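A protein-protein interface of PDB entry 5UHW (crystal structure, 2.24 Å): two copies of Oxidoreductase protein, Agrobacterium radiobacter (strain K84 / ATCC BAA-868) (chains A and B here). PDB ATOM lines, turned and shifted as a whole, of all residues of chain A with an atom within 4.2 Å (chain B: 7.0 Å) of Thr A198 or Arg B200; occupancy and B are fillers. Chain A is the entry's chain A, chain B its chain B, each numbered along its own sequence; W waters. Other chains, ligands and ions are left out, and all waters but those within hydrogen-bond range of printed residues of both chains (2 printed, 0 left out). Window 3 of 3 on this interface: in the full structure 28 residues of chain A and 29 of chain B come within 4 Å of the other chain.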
ATOM      1  N   LEU A 197      -1.291   7.254 -26.714  1.00  0.00           N
ATOM      2  CA  LEU A 197      -1.445   6.226 -27.707  1.00  0.00           C
ATOM      3  C   LEU A 197      -0.596   6.546 -28.932  1.00  0.00           C
ATOM      4  O   LEU A 197      -0.562   7.691 -29.376  1.00  0.00           O
ATOM      5  CB  LEU A 197      -2.916   6.182 -28.101  1.00  0.00           C
ATOM      6  CG  LEU A 197      -3.374   5.153 -29.137  1.00  0.00           C
ATOM      7  CD1 LEU A 197      -4.759   4.604 -28.814  1.00  0.00           C
ATOM      8  CD2 LEU A 197      -3.369   5.718 -30.556  1.00  0.00           C
ATOM      9  N   THR A 198       0.042   5.528 -29.501  1.00  0.00           N
ATOM     10  CA  THR A 198       0.731   5.643 -30.799  1.00  0.00           C
ATOM     11  C   THR A 198       0.315   4.476 -31.704  1.00  0.00           C
ATOM     12  O   THR A 198       0.264   3.341 -31.253  1.00  0.00           O
ATOM     13  CB  THR A 198       2.277   5.657 -30.636  1.00  0.00           C
ATOM     14  OG1 THR A 198       2.666   6.395 -29.459  1.00  0.00           O
ATOM     15  CG2 THR A 198       2.913   6.294 -31.833  1.00  0.00           C
ATOM     16  N   ALA A 199       0.026   4.759 -32.973  1.00  0.00           N
ATOM     17  CA  ALA A 199      -0.636   3.799 -33.881  1.00  0.00           C
ATOM     18  C   ALA A 199      -0.048   3.799 -35.274  1.00  0.00           C
ATOM     19  O   ALA A 199       0.365   4.835 -35.758  1.00  0.00           O
ATOM     20  CB  ALA A 199      -2.115   4.129 -33.984  1.00  0.00           C
ATOM     21  N   ARG A 200      -0.040   2.641 -35.931  1.00  0.00           N
ATOM     22  CA  ARG A 200       0.431   2.527 -37.319  1.00  0.00           C
ATOM     23  C   ARG A 200      -0.572   1.674 -38.053  1.00  0.00           C
ATOM     24  O   ARG A 200      -1.136   0.752 -37.468  1.00  0.00           O
ATOM     25  CB  ARG A 200       1.820   1.894 -37.395  1.00  0.00           C
ATOM     26  CG  ARG A 200       2.907   2.644 -36.651  1.00  0.00           C
ATOM     27  CD  ARG A 200       3.212   3.991 -37.272  1.00  0.00           C
ATOM     28  NE  ARG A 200       4.426   4.580 -36.699  1.00  0.00           N
ATOM     29  CZ  ARG A 200       4.476   5.478 -35.711  1.00  0.00           C
ATOM     30  NH1 ARG A 200       3.379   5.987 -35.165  1.00  0.00           N
ATOM     31  NH2 ARG A 200       5.656   5.891 -35.269  1.00  0.00           N
ATOM     32  N   THR A 215      -1.274  -1.550 -35.578  1.00  0.00           N
ATOM     33  CA  THR A 215      -0.407  -1.872 -34.453  1.00  0.00           C
ATOM     34  C   THR A 215      -0.387  -0.625 -33.581  1.00  0.00           C
ATOM     35  O   THR A 215      -0.071   0.444 -34.053  1.00  0.00           O
ATOM     36  CB  THR A 215       1.025  -2.262 -34.916  1.00  0.00           C
ATOM     37  OG1 THR A 215       0.960  -3.268 -35.940  1.00  0.00           O
ATOM     38  CG2 THR A 215       1.851  -2.792 -33.745  1.00  0.00           C
ATOM     39  N   ILE A 216      -0.743  -0.784 -32.312  1.00  0.00           N
ATOM     40  CA  ILE A 216      -1.007   0.336 -31.413  1.00  0.00           C
ATOM     41  C   ILE A 216      -0.238   0.105 -30.107  1.00  0.00           C
ATOM     42  O   ILE A 216      -0.276  -0.986 -29.547  1.00  0.00           O
ATOM     43  CB  ILE A 216      -2.530   0.508 -31.160  1.00  0.00           C
ATOM     44  CG1 ILE A 216      -3.299   0.625 -32.475  1.00  0.00           C
ATOM     45  CG2 ILE A 216      -2.812   1.751 -30.331  1.00  0.00           C
ATOM     46  CD1 ILE A 216      -4.797   0.480 -32.352  1.00  0.00           C
ATOM     47  N   LEU A 217       0.502   1.128 -29.682  1.00  0.00           N
ATOM     48  CA  LEU A 217       1.256   1.122 -28.442  1.00  0.00           C
ATOM     49  C   LEU A 217       0.546   2.017 -27.439  1.00  0.00           C
ATOM     50  O   LEU A 217       0.309   3.179 -27.733  1.00  0.00           O
ATOM     51  CB  LEU A 217       2.632   1.683 -28.706  1.00  0.00           C
ATOM     52  CG  LEU A 217       3.647   1.750 -27.569  1.00  0.00           C
ATOM     53  CD1 LEU A 217       3.930   0.369 -27.033  1.00  0.00           C
ATOM     54  CD2 LEU A 217       4.939   2.363 -28.096  1.00  0.00           C
ATOM     55  N   ASP A 219       0.207   3.671 -23.525  1.00  0.00           N
ATOM     56  CA  ASP A 219       0.748   3.979 -22.186  1.00  0.00           C
ATOM     57  C   ASP A 219      -0.463   4.134 -21.264  1.00  0.00           C
ATOM     58  O   ASP A 219      -1.229   5.109 -21.392  1.00  0.00           O
ATOM     59  CB  ASP A 219       1.607   5.236 -22.215  1.00  0.00           C
ATOM     60  CG  ASP A 219       2.575   5.232 -23.382  1.00  0.00           C
ATOM     61  OD1 ASP A 219       3.426   4.313 -23.425  1.00  0.00           O
ATOM     62  OD2 ASP A 219       2.466   6.102 -24.283  1.00  0.00           O
ATOM     63  N   SER A 332      -3.159   9.353 -34.966  1.00  0.00           N
ATOM     64  CA  SER A 332      -1.742   8.963 -34.809  1.00  0.00           C
ATOM     65  C   SER A 332      -1.177   8.362 -36.090  1.00  0.00           C
ATOM     66  O   SER A 332      -0.118   8.737 -36.530  1.00  0.00           O
ATOM     67  CB  SER A 332      -1.581   7.956 -33.665  1.00  0.00           C
ATOM     68  OG  SER A 332      -0.218   7.677 -33.411  1.00  0.00           O
ATOM     69  N   THR A 338       2.380  10.604 -31.552  1.00  0.00           N
ATOM     70  CA  THR A 338       1.733  10.181 -30.307  1.00  0.00           C
ATOM     71  C   THR A 338       0.633  11.164 -29.876  1.00  0.00           C
ATOM     72  O   THR A 338       0.793  12.365 -30.013  1.00  0.00           O
ATOM     73  CB  THR A 338       2.785  10.014 -29.207  1.00  0.00           C
ATOM     74  OG1 THR A 338       3.699   8.989 -29.612  1.00  0.00           O
ATOM     75  CG2 THR A 338       2.159   9.617 -27.890  1.00  0.00           C
ATOM     76  N   ILE B 176      18.188  -2.729 -22.659  1.00  0.00           N
ATOM     77  CA  ILE B 176      18.355  -2.402 -24.088  1.00  0.00           C
ATOM     78  C   ILE B 176      19.822  -2.494 -24.536  1.00  0.00           C
ATOM     79  O   ILE B 176      20.120  -3.039 -25.587  1.00  0.00           O
ATOM     80  CB  ILE B 176      17.793  -1.031 -24.487  1.00  0.00           C
ATOM     81  CG1 ILE B 176      16.364  -0.845 -23.980  1.00  0.00           C
ATOM     82  CG2 ILE B 176      17.808  -0.899 -26.011  1.00  0.00           C
ATOM     83  CD1 ILE B 176      15.733   0.456 -24.428  1.00  0.00           C
ATOM     84  N   THR B 198       9.857   4.259 -31.873  1.00  0.00           N
ATOM     85  CA  THR B 198       9.241   4.749 -30.612  1.00  0.00           C
ATOM     86  C   THR B 198       9.397   3.716 -29.506  1.00  0.00           C
ATOM     87  O   THR B 198       9.053   2.563 -29.723  1.00  0.00           O
ATOM     88  CB  THR B 198       7.740   5.007 -30.755  1.00  0.00           C
ATOM     89  OG1 THR B 198       7.462   5.517 -32.056  1.00  0.00           O
ATOM     90  CG2 THR B 198       7.288   6.012 -29.726  1.00  0.00           C
ATOM     91  N   ALA B 199       9.849   4.123 -28.318  1.00  0.00           N
ATOM     92  CA  ALA B 199      10.126   3.182 -27.225  1.00  0.00           C
ATOM     93  C   ALA B 199       9.604   3.609 -25.868  1.00  0.00           C
ATOM     94  O   ALA B 199       9.405   4.779 -25.615  1.00  0.00           O
ATOM     95  CB  ALA B 199      11.615   2.959 -27.113  1.00  0.00           C
ATOM     96  N   ARG B 200       9.410   2.621 -24.998  1.00  0.00           N
ATOM     97  CA  ARG B 200       9.015   2.817 -23.614  1.00  0.00           C
ATOM     98  C   ARG B 200       9.858   1.907 -22.754  1.00  0.00           C
ATOM     99  O   ARG B 200      10.147   0.796 -23.162  1.00  0.00           O
ATOM    100  CB  ARG B 200       7.563   2.435 -23.429  1.00  0.00           C
ATOM    101  CG  ARG B 200       6.601   3.237 -24.271  1.00  0.00           C
ATOM    102  CD  ARG B 200       6.549   4.714 -23.882  1.00  0.00           C
ATOM    103  NE  ARG B 200       5.561   5.401 -24.718  1.00  0.00           N
ATOM    104  CZ  ARG B 200       5.819   6.167 -25.775  1.00  0.00           C
ATOM    105  NH1 ARG B 200       7.053   6.403 -26.186  1.00  0.00           N
ATOM    106  NH2 ARG B 200       4.805   6.701 -26.449  1.00  0.00           N
ATOM    107  N   THR B 201      10.258   2.367 -21.576  1.00  0.00           N
ATOM    108  CA  THR B 201      10.988   1.528 -20.647  1.00  0.00           C
ATOM    109  C   THR B 201      10.427   1.631 -19.231  1.00  0.00           C
ATOM    110  O   THR B 201       9.731   2.572 -18.889  1.00  0.00           O
ATOM    111  CB  THR B 201      12.503   1.816 -20.675  1.00  0.00           C
ATOM    112  OG1 THR B 201      12.793   3.168 -20.295  1.00  0.00           O
ATOM    113  CG2 THR B 201      13.068   1.569 -22.061  1.00  0.00           C
ATOM    114  N   LYS B 202      10.724   0.612 -18.435  1.00  0.00           N
ATOM    115  CA  LYS B 202      10.177   0.439 -17.098  1.00  0.00           C
ATOM    116  C   LYS B 202      11.212  -0.323 -16.284  1.00  0.00           C
ATOM    117  O   LYS B 202      11.915  -1.184 -16.828  1.00  0.00           O
ATOM    118  CB  LYS B 202       8.874  -0.363 -17.168  1.00  0.00           C
ATOM    119  CG  LYS B 202       7.780   0.089 -16.223  1.00  0.00           C
ATOM    120  CD  LYS B 202       6.408  -0.455 -16.600  1.00  0.00           C
ATOM    121  CE  LYS B 202       5.947   0.004 -17.990  1.00  0.00           C
ATOM    122  NZ  LYS B 202       6.371  -0.901 -19.124  1.00  0.00           N
ATOM    123  N   GLU B 211      16.672  -0.039 -16.403  1.00  0.00           N
ATOM    124  CA  GLU B 211      15.376  -0.530 -16.939  1.00  0.00           C
ATOM    125  C   GLU B 211      15.483  -2.009 -17.328  1.00  0.00           C
ATOM    126  O   GLU B 211      16.475  -2.425 -17.946  1.00  0.00           O
ATOM    127  CB  GLU B 211      14.900   0.339 -18.126  1.00  0.00           C
ATOM    128  CG  GLU B 211      15.435  -0.012 -19.519  1.00  0.00           C
ATOM    129  CD  GLU B 211      16.948   0.091 -19.691  1.00  0.00           C
ATOM    130  OE1 GLU B 211      17.630   0.736 -18.847  1.00  0.00           O
ATOM    131  OE2 GLU B 211      17.461  -0.472 -20.699  1.00  0.00           O
ATOM    132  N   VAL B 213      12.520  -3.733 -18.621  1.00  0.00           N
ATOM    133  CA  VAL B 213      11.465  -3.976 -19.591  1.00  0.00           C
ATOM    134  C   VAL B 213      11.561  -2.868 -20.611  1.00  0.00           C
ATOM    135  O   VAL B 213      11.710  -1.699 -20.240  1.00  0.00           O
ATOM    136  CB  VAL B 213      10.081  -3.958 -18.935  1.00  0.00           C
ATOM    137  CG1 VAL B 213       8.981  -4.278 -19.955  1.00  0.00           C
ATOM    138  CG2 VAL B 213      10.047  -4.937 -17.763  1.00  0.00           C
ATOM    139  N   ALA B 214      11.525  -3.232 -21.892  1.00  0.00           N
ATOM    140  CA  ALA B 214      11.523  -2.253 -22.977  1.00  0.00           C
ATOM    141  C   ALA B 214      10.619  -2.751 -24.087  1.00  0.00           C
ATOM    142  O   ALA B 214      10.727  -3.892 -24.499  1.00  0.00           O
ATOM    143  CB  ALA B 214      12.925  -2.016 -23.497  1.00  0.00           C
ATOM    144  N   THR B 215       9.704  -1.897 -24.535  1.00  0.00           N
ATOM    145  CA  THR B 215       8.806  -2.200 -25.643  1.00  0.00           C
ATOM    146  C   THR B 215       9.082  -1.145 -26.734  1.00  0.00           C
ATOM    147  O   THR B 215       9.015   0.044 -26.457  1.00  0.00           O
ATOM    148  CB  THR B 215       7.330  -2.197 -25.187  1.00  0.00           C
ATOM    149  OG1 THR B 215       7.168  -3.066 -24.052  1.00  0.00           O
ATOM    150  CG2 THR B 215       6.408  -2.638 -26.306  1.00  0.00           C
ATOM    151  N   ILE B 216       9.407  -1.593 -27.953  1.00  0.00           N
ATOM    152  CA  ILE B 216       9.820  -0.706 -29.044  1.00  0.00           C
ATOM    153  C   ILE B 216       8.988  -0.959 -30.308  1.00  0.00           C
ATOM    154  O   ILE B 216       8.758  -2.105 -30.678  1.00  0.00           O
ATOM    155  CB  ILE B 216      11.318  -0.892 -29.367  1.00  0.00           C
ATOM    156  CG1 ILE B 216      12.159  -0.658 -28.102  1.00  0.00           C
ATOM    157  CG2 ILE B 216      11.746   0.032 -30.511  1.00  0.00           C
ATOM    158  CD1 ILE B 216      13.590  -1.113 -28.204  1.00  0.00           C
ATOM    159  N   LEU B 217       8.558   0.129 -30.954  1.00  0.00           N
ATOM    160  CA  LEU B 217       7.759   0.095 -32.182  1.00  0.00           C
ATOM    161  C   LEU B 217       8.617   0.619 -33.351  1.00  0.00           C
ATOM    162  O   LEU B 217       9.074   1.770 -33.339  1.00  0.00           O
ATOM    163  CB  LEU B 217       6.512   0.959 -31.989  1.00  0.00           C
ATOM    164  CG  LEU B 217       5.589   1.167 -33.194  1.00  0.00           C
ATOM    165  CD1 LEU B 217       4.889  -0.135 -33.557  1.00  0.00           C
ATOM    166  CD2 LEU B 217       4.564   2.266 -32.938  1.00  0.00           C
ATOM    167  N   ALA B 329      16.312   4.497 -28.828  1.00  0.00           N
ATOM    168  CA  ALA B 329      15.306   3.948 -27.920  1.00  0.00           C
ATOM    169  C   ALA B 329      15.396   4.595 -26.546  1.00  0.00           C
ATOM    170  O   ALA B 329      14.380   5.004 -25.970  1.00  0.00           O
ATOM    171  CB  ALA B 329      15.437   2.437 -27.826  1.00  0.00           C
ATOM    172  N   SER B 332      14.028   8.106 -27.042  1.00  0.00           N
ATOM    173  CA  SER B 332      12.561   8.046 -27.186  1.00  0.00           C
ATOM    174  C   SER B 332      11.826   7.821 -25.851  1.00  0.00           C
ATOM    175  O   SER B 332      10.880   8.555 -25.530  1.00  0.00           O
ATOM    176  CB  SER B 332      12.190   6.944 -28.194  1.00  0.00           C
ATOM    177  OG  SER B 332      10.793   6.818 -28.341  1.00  0.00           O
ATOM    178  N   ALA B 333      12.280   6.820 -25.084  1.00  0.00           N
ATOM    179  CA  ALA B 333      11.720   6.498 -23.749  1.00  0.00           C
ATOM    180  C   ALA B 333      11.787   7.655 -22.724  1.00  0.00           C
ATOM    181  O   ALA B 333      10.934   7.762 -21.873  1.00  0.00           O
ATOM    182  CB  ALA B 333      12.399   5.258 -23.179  1.00  0.00           C
ATOM    183  N   ALA B 334      12.811   8.501 -22.813  1.00  0.00           N
ATOM    184  CA  ALA B 334      12.950   9.676 -21.940  1.00  0.00           C
ATOM    185  C   ALA B 334      12.107  10.846 -22.451  1.00  0.00           C
ATOM    186  O   ALA B 334      11.417  11.480 -21.671  1.00  0.00           O
ATOM    187  CB  ALA B 334      14.415  10.077 -21.823  1.00  0.00           C
ATOM    188  N   ASN B 335      12.181  11.127 -23.758  1.00  0.00           N
ATOM    189  CA  ASN B 335      11.411  12.222 -24.418  1.00  0.00           C
ATOM    190  C   ASN B 335       9.932  11.943 -24.397  1.00  0.00           C
ATOM    191  O   ASN B 335       9.148  12.853 -24.215  1.00  0.00           O
ATOM    192  CB  ASN B 335      11.760  12.372 -25.928  1.00  0.00           C
ATOM    193  CG  ASN B 335      13.151  12.938 -26.199  1.00  0.00           C
ATOM    194  OD1 ASN B 335      13.897  13.320 -25.284  1.00  0.00           O
ATOM    195  ND2 ASN B 335      13.516  12.984 -27.490  1.00  0.00           N
ATOM    196  N   GLY B 336       9.566  10.684 -24.646  1.00  0.00           N
ATOM    197  CA  GLY B 336       8.204  10.315 -25.021  1.00  0.00           C
ATOM    198  C   GLY B 336       7.974  10.440 -26.521  1.00  0.00           C
ATOM    199  O   GLY B 336       6.859  10.255 -26.989  1.00  0.00           O
ATOM    200  N   ARG B 337       9.032  10.679 -27.292  1.00  0.00           N
ATOM    201  CA  ARG B 337       8.903  11.125 -28.681  1.00  0.00           C
ATOM    202  C   ARG B 337       9.365  10.027 -29.657  1.00  0.00           C
ATOM    203  O   ARG B 337      10.223   9.228 -29.316  1.00  0.00           O
ATOM    204  CB  ARG B 337       9.705  12.438 -28.873  1.00  0.00           C
ATOM    205  N   THR B 338       8.766   9.971 -30.851  1.00  0.00           N
ATOM    206  CA  THR B 338       9.289   9.161 -31.974  1.00  0.00           C
ATOM    207  C   THR B 338      10.601   9.768 -32.467  1.00  0.00           C
ATOM    208  O   THR B 338      10.663  10.959 -32.684  1.00  0.00           O
ATOM    209  CB  THR B 338       8.308   9.139 -33.178  1.00  0.00           C
ATOM    210  OG1 THR B 338       7.081   8.523 -32.801  1.00  0.00           O
ATOM    211  CG2 THR B 338       8.871   8.349 -34.350  1.00  0.00           C
HETATM  212  O   HOH W   1       8.064   4.037 -34.358  1.00  0.00           O
HETATM  213  O   HOH W   2       1.816   5.428 -26.955  1.00  0.00           O
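Of the 20 printed residues of chain B, 4 touch a printed residue of chain A.
Printed residues of chain B that touch a printed residue of chain A: Thr B198, Arg B200, Thr B215 and Thr B338.
Along chain A the printed residues that touch a printed residue of chain B span positions 198 to 219.
Among the printed residues, 5 pairs touch across the chains.
Water W1 lies within hydrogen-bond range of the backbone carbonyl oxygen of Leu B217 (2.7 Å), the side-chain hydroxyl of Thr B198 (2.8 Å) and the guanidinium group of Arg A200 (3.2 Å).
Water W2 lies within hydrogen-bond range of the side-chain hydroxyl (OG1) of Thr A198 (2.8 Å), the backbone carbonyl oxygen (O) of Leu A217 (2.8 Å), the side-chain carboxylate (OD2) of Asp A219 (2.8 Å) and the guanidinium group (NH2) of Arg B200 (3.3 Å).
The guanidinium group (NE) of Arg B200 lies within salt-bridge range of the side-chain carboxylate (OD1) of Asp A219, 2.7 Å away.
Thr A198 touches just one residue of chain B: Arg B200.
Of chain A, only Thr A198 (3.7 Å) and Asp A219 (2.7 Å) come within 4 Å of Arg B200.
Printed residues of chain A within 4 Å of Thr B198: Arg A200.
Of the printed residues of chain B, Leu A217 touches Thr B215 (3.96 Å).
Printed residues of chain B within 4 Å of Asp A219: Arg B200 (2.7 Å).
Of the printed residues of chain B, Arg A200 touches Thr B198 (3.7 Å) and Thr B338 (3.9 Å).
Val B213 touches none of the printed residues of chain A.
Thr A198 touches Arg B200, and with the chains exchanged Arg A200 touches Thr B198.
Arg A200 touches Thr B338, but with the chains exchanged Thr A338 does not touch Arg B200 (4.1 Å).
Leu A217 touches Thr B215, but with the chains exchanged Thr A215 does not touch Leu B217 (4.04 Å).
The backbone NH (N) of Arg A200 sits at hydrogen-bond distance from the backbone carbonyl oxygen (O) of Thr A215 (2.9 Å).
OG1 of Thr A198 is in hydrogen-bond range of OG1 of Thr A338 (2.8 Å).
The backbone carbonyl oxygen (O) of Thr A198 is in hydrogen-bond range of the backbone NH (N) of Leu A217 (2.7 Å).
The backbone carbonyl oxygen (O) of Thr B215 lies within hydrogen-bond range of the backbone NH (N) of Arg B200.
O of Thr B198 lies within hydrogen-bond range of N of Leu B217, at 2.8 Å.
The side-chain hydroxyl of Thr B338 sits at hydrogen-bond distance from the side-chain hydroxyl of Thr B198 (3.1 Å).
Among the printed residues, pairs that only touch across the chains: Thr A198 with Arg B200 (3.7 Å), Arg A200 with Thr B198 (3.7 Å), Arg A200 with Thr B338 (3.9 Å) and Leu A217 with Thr B215 (3.96 Å).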
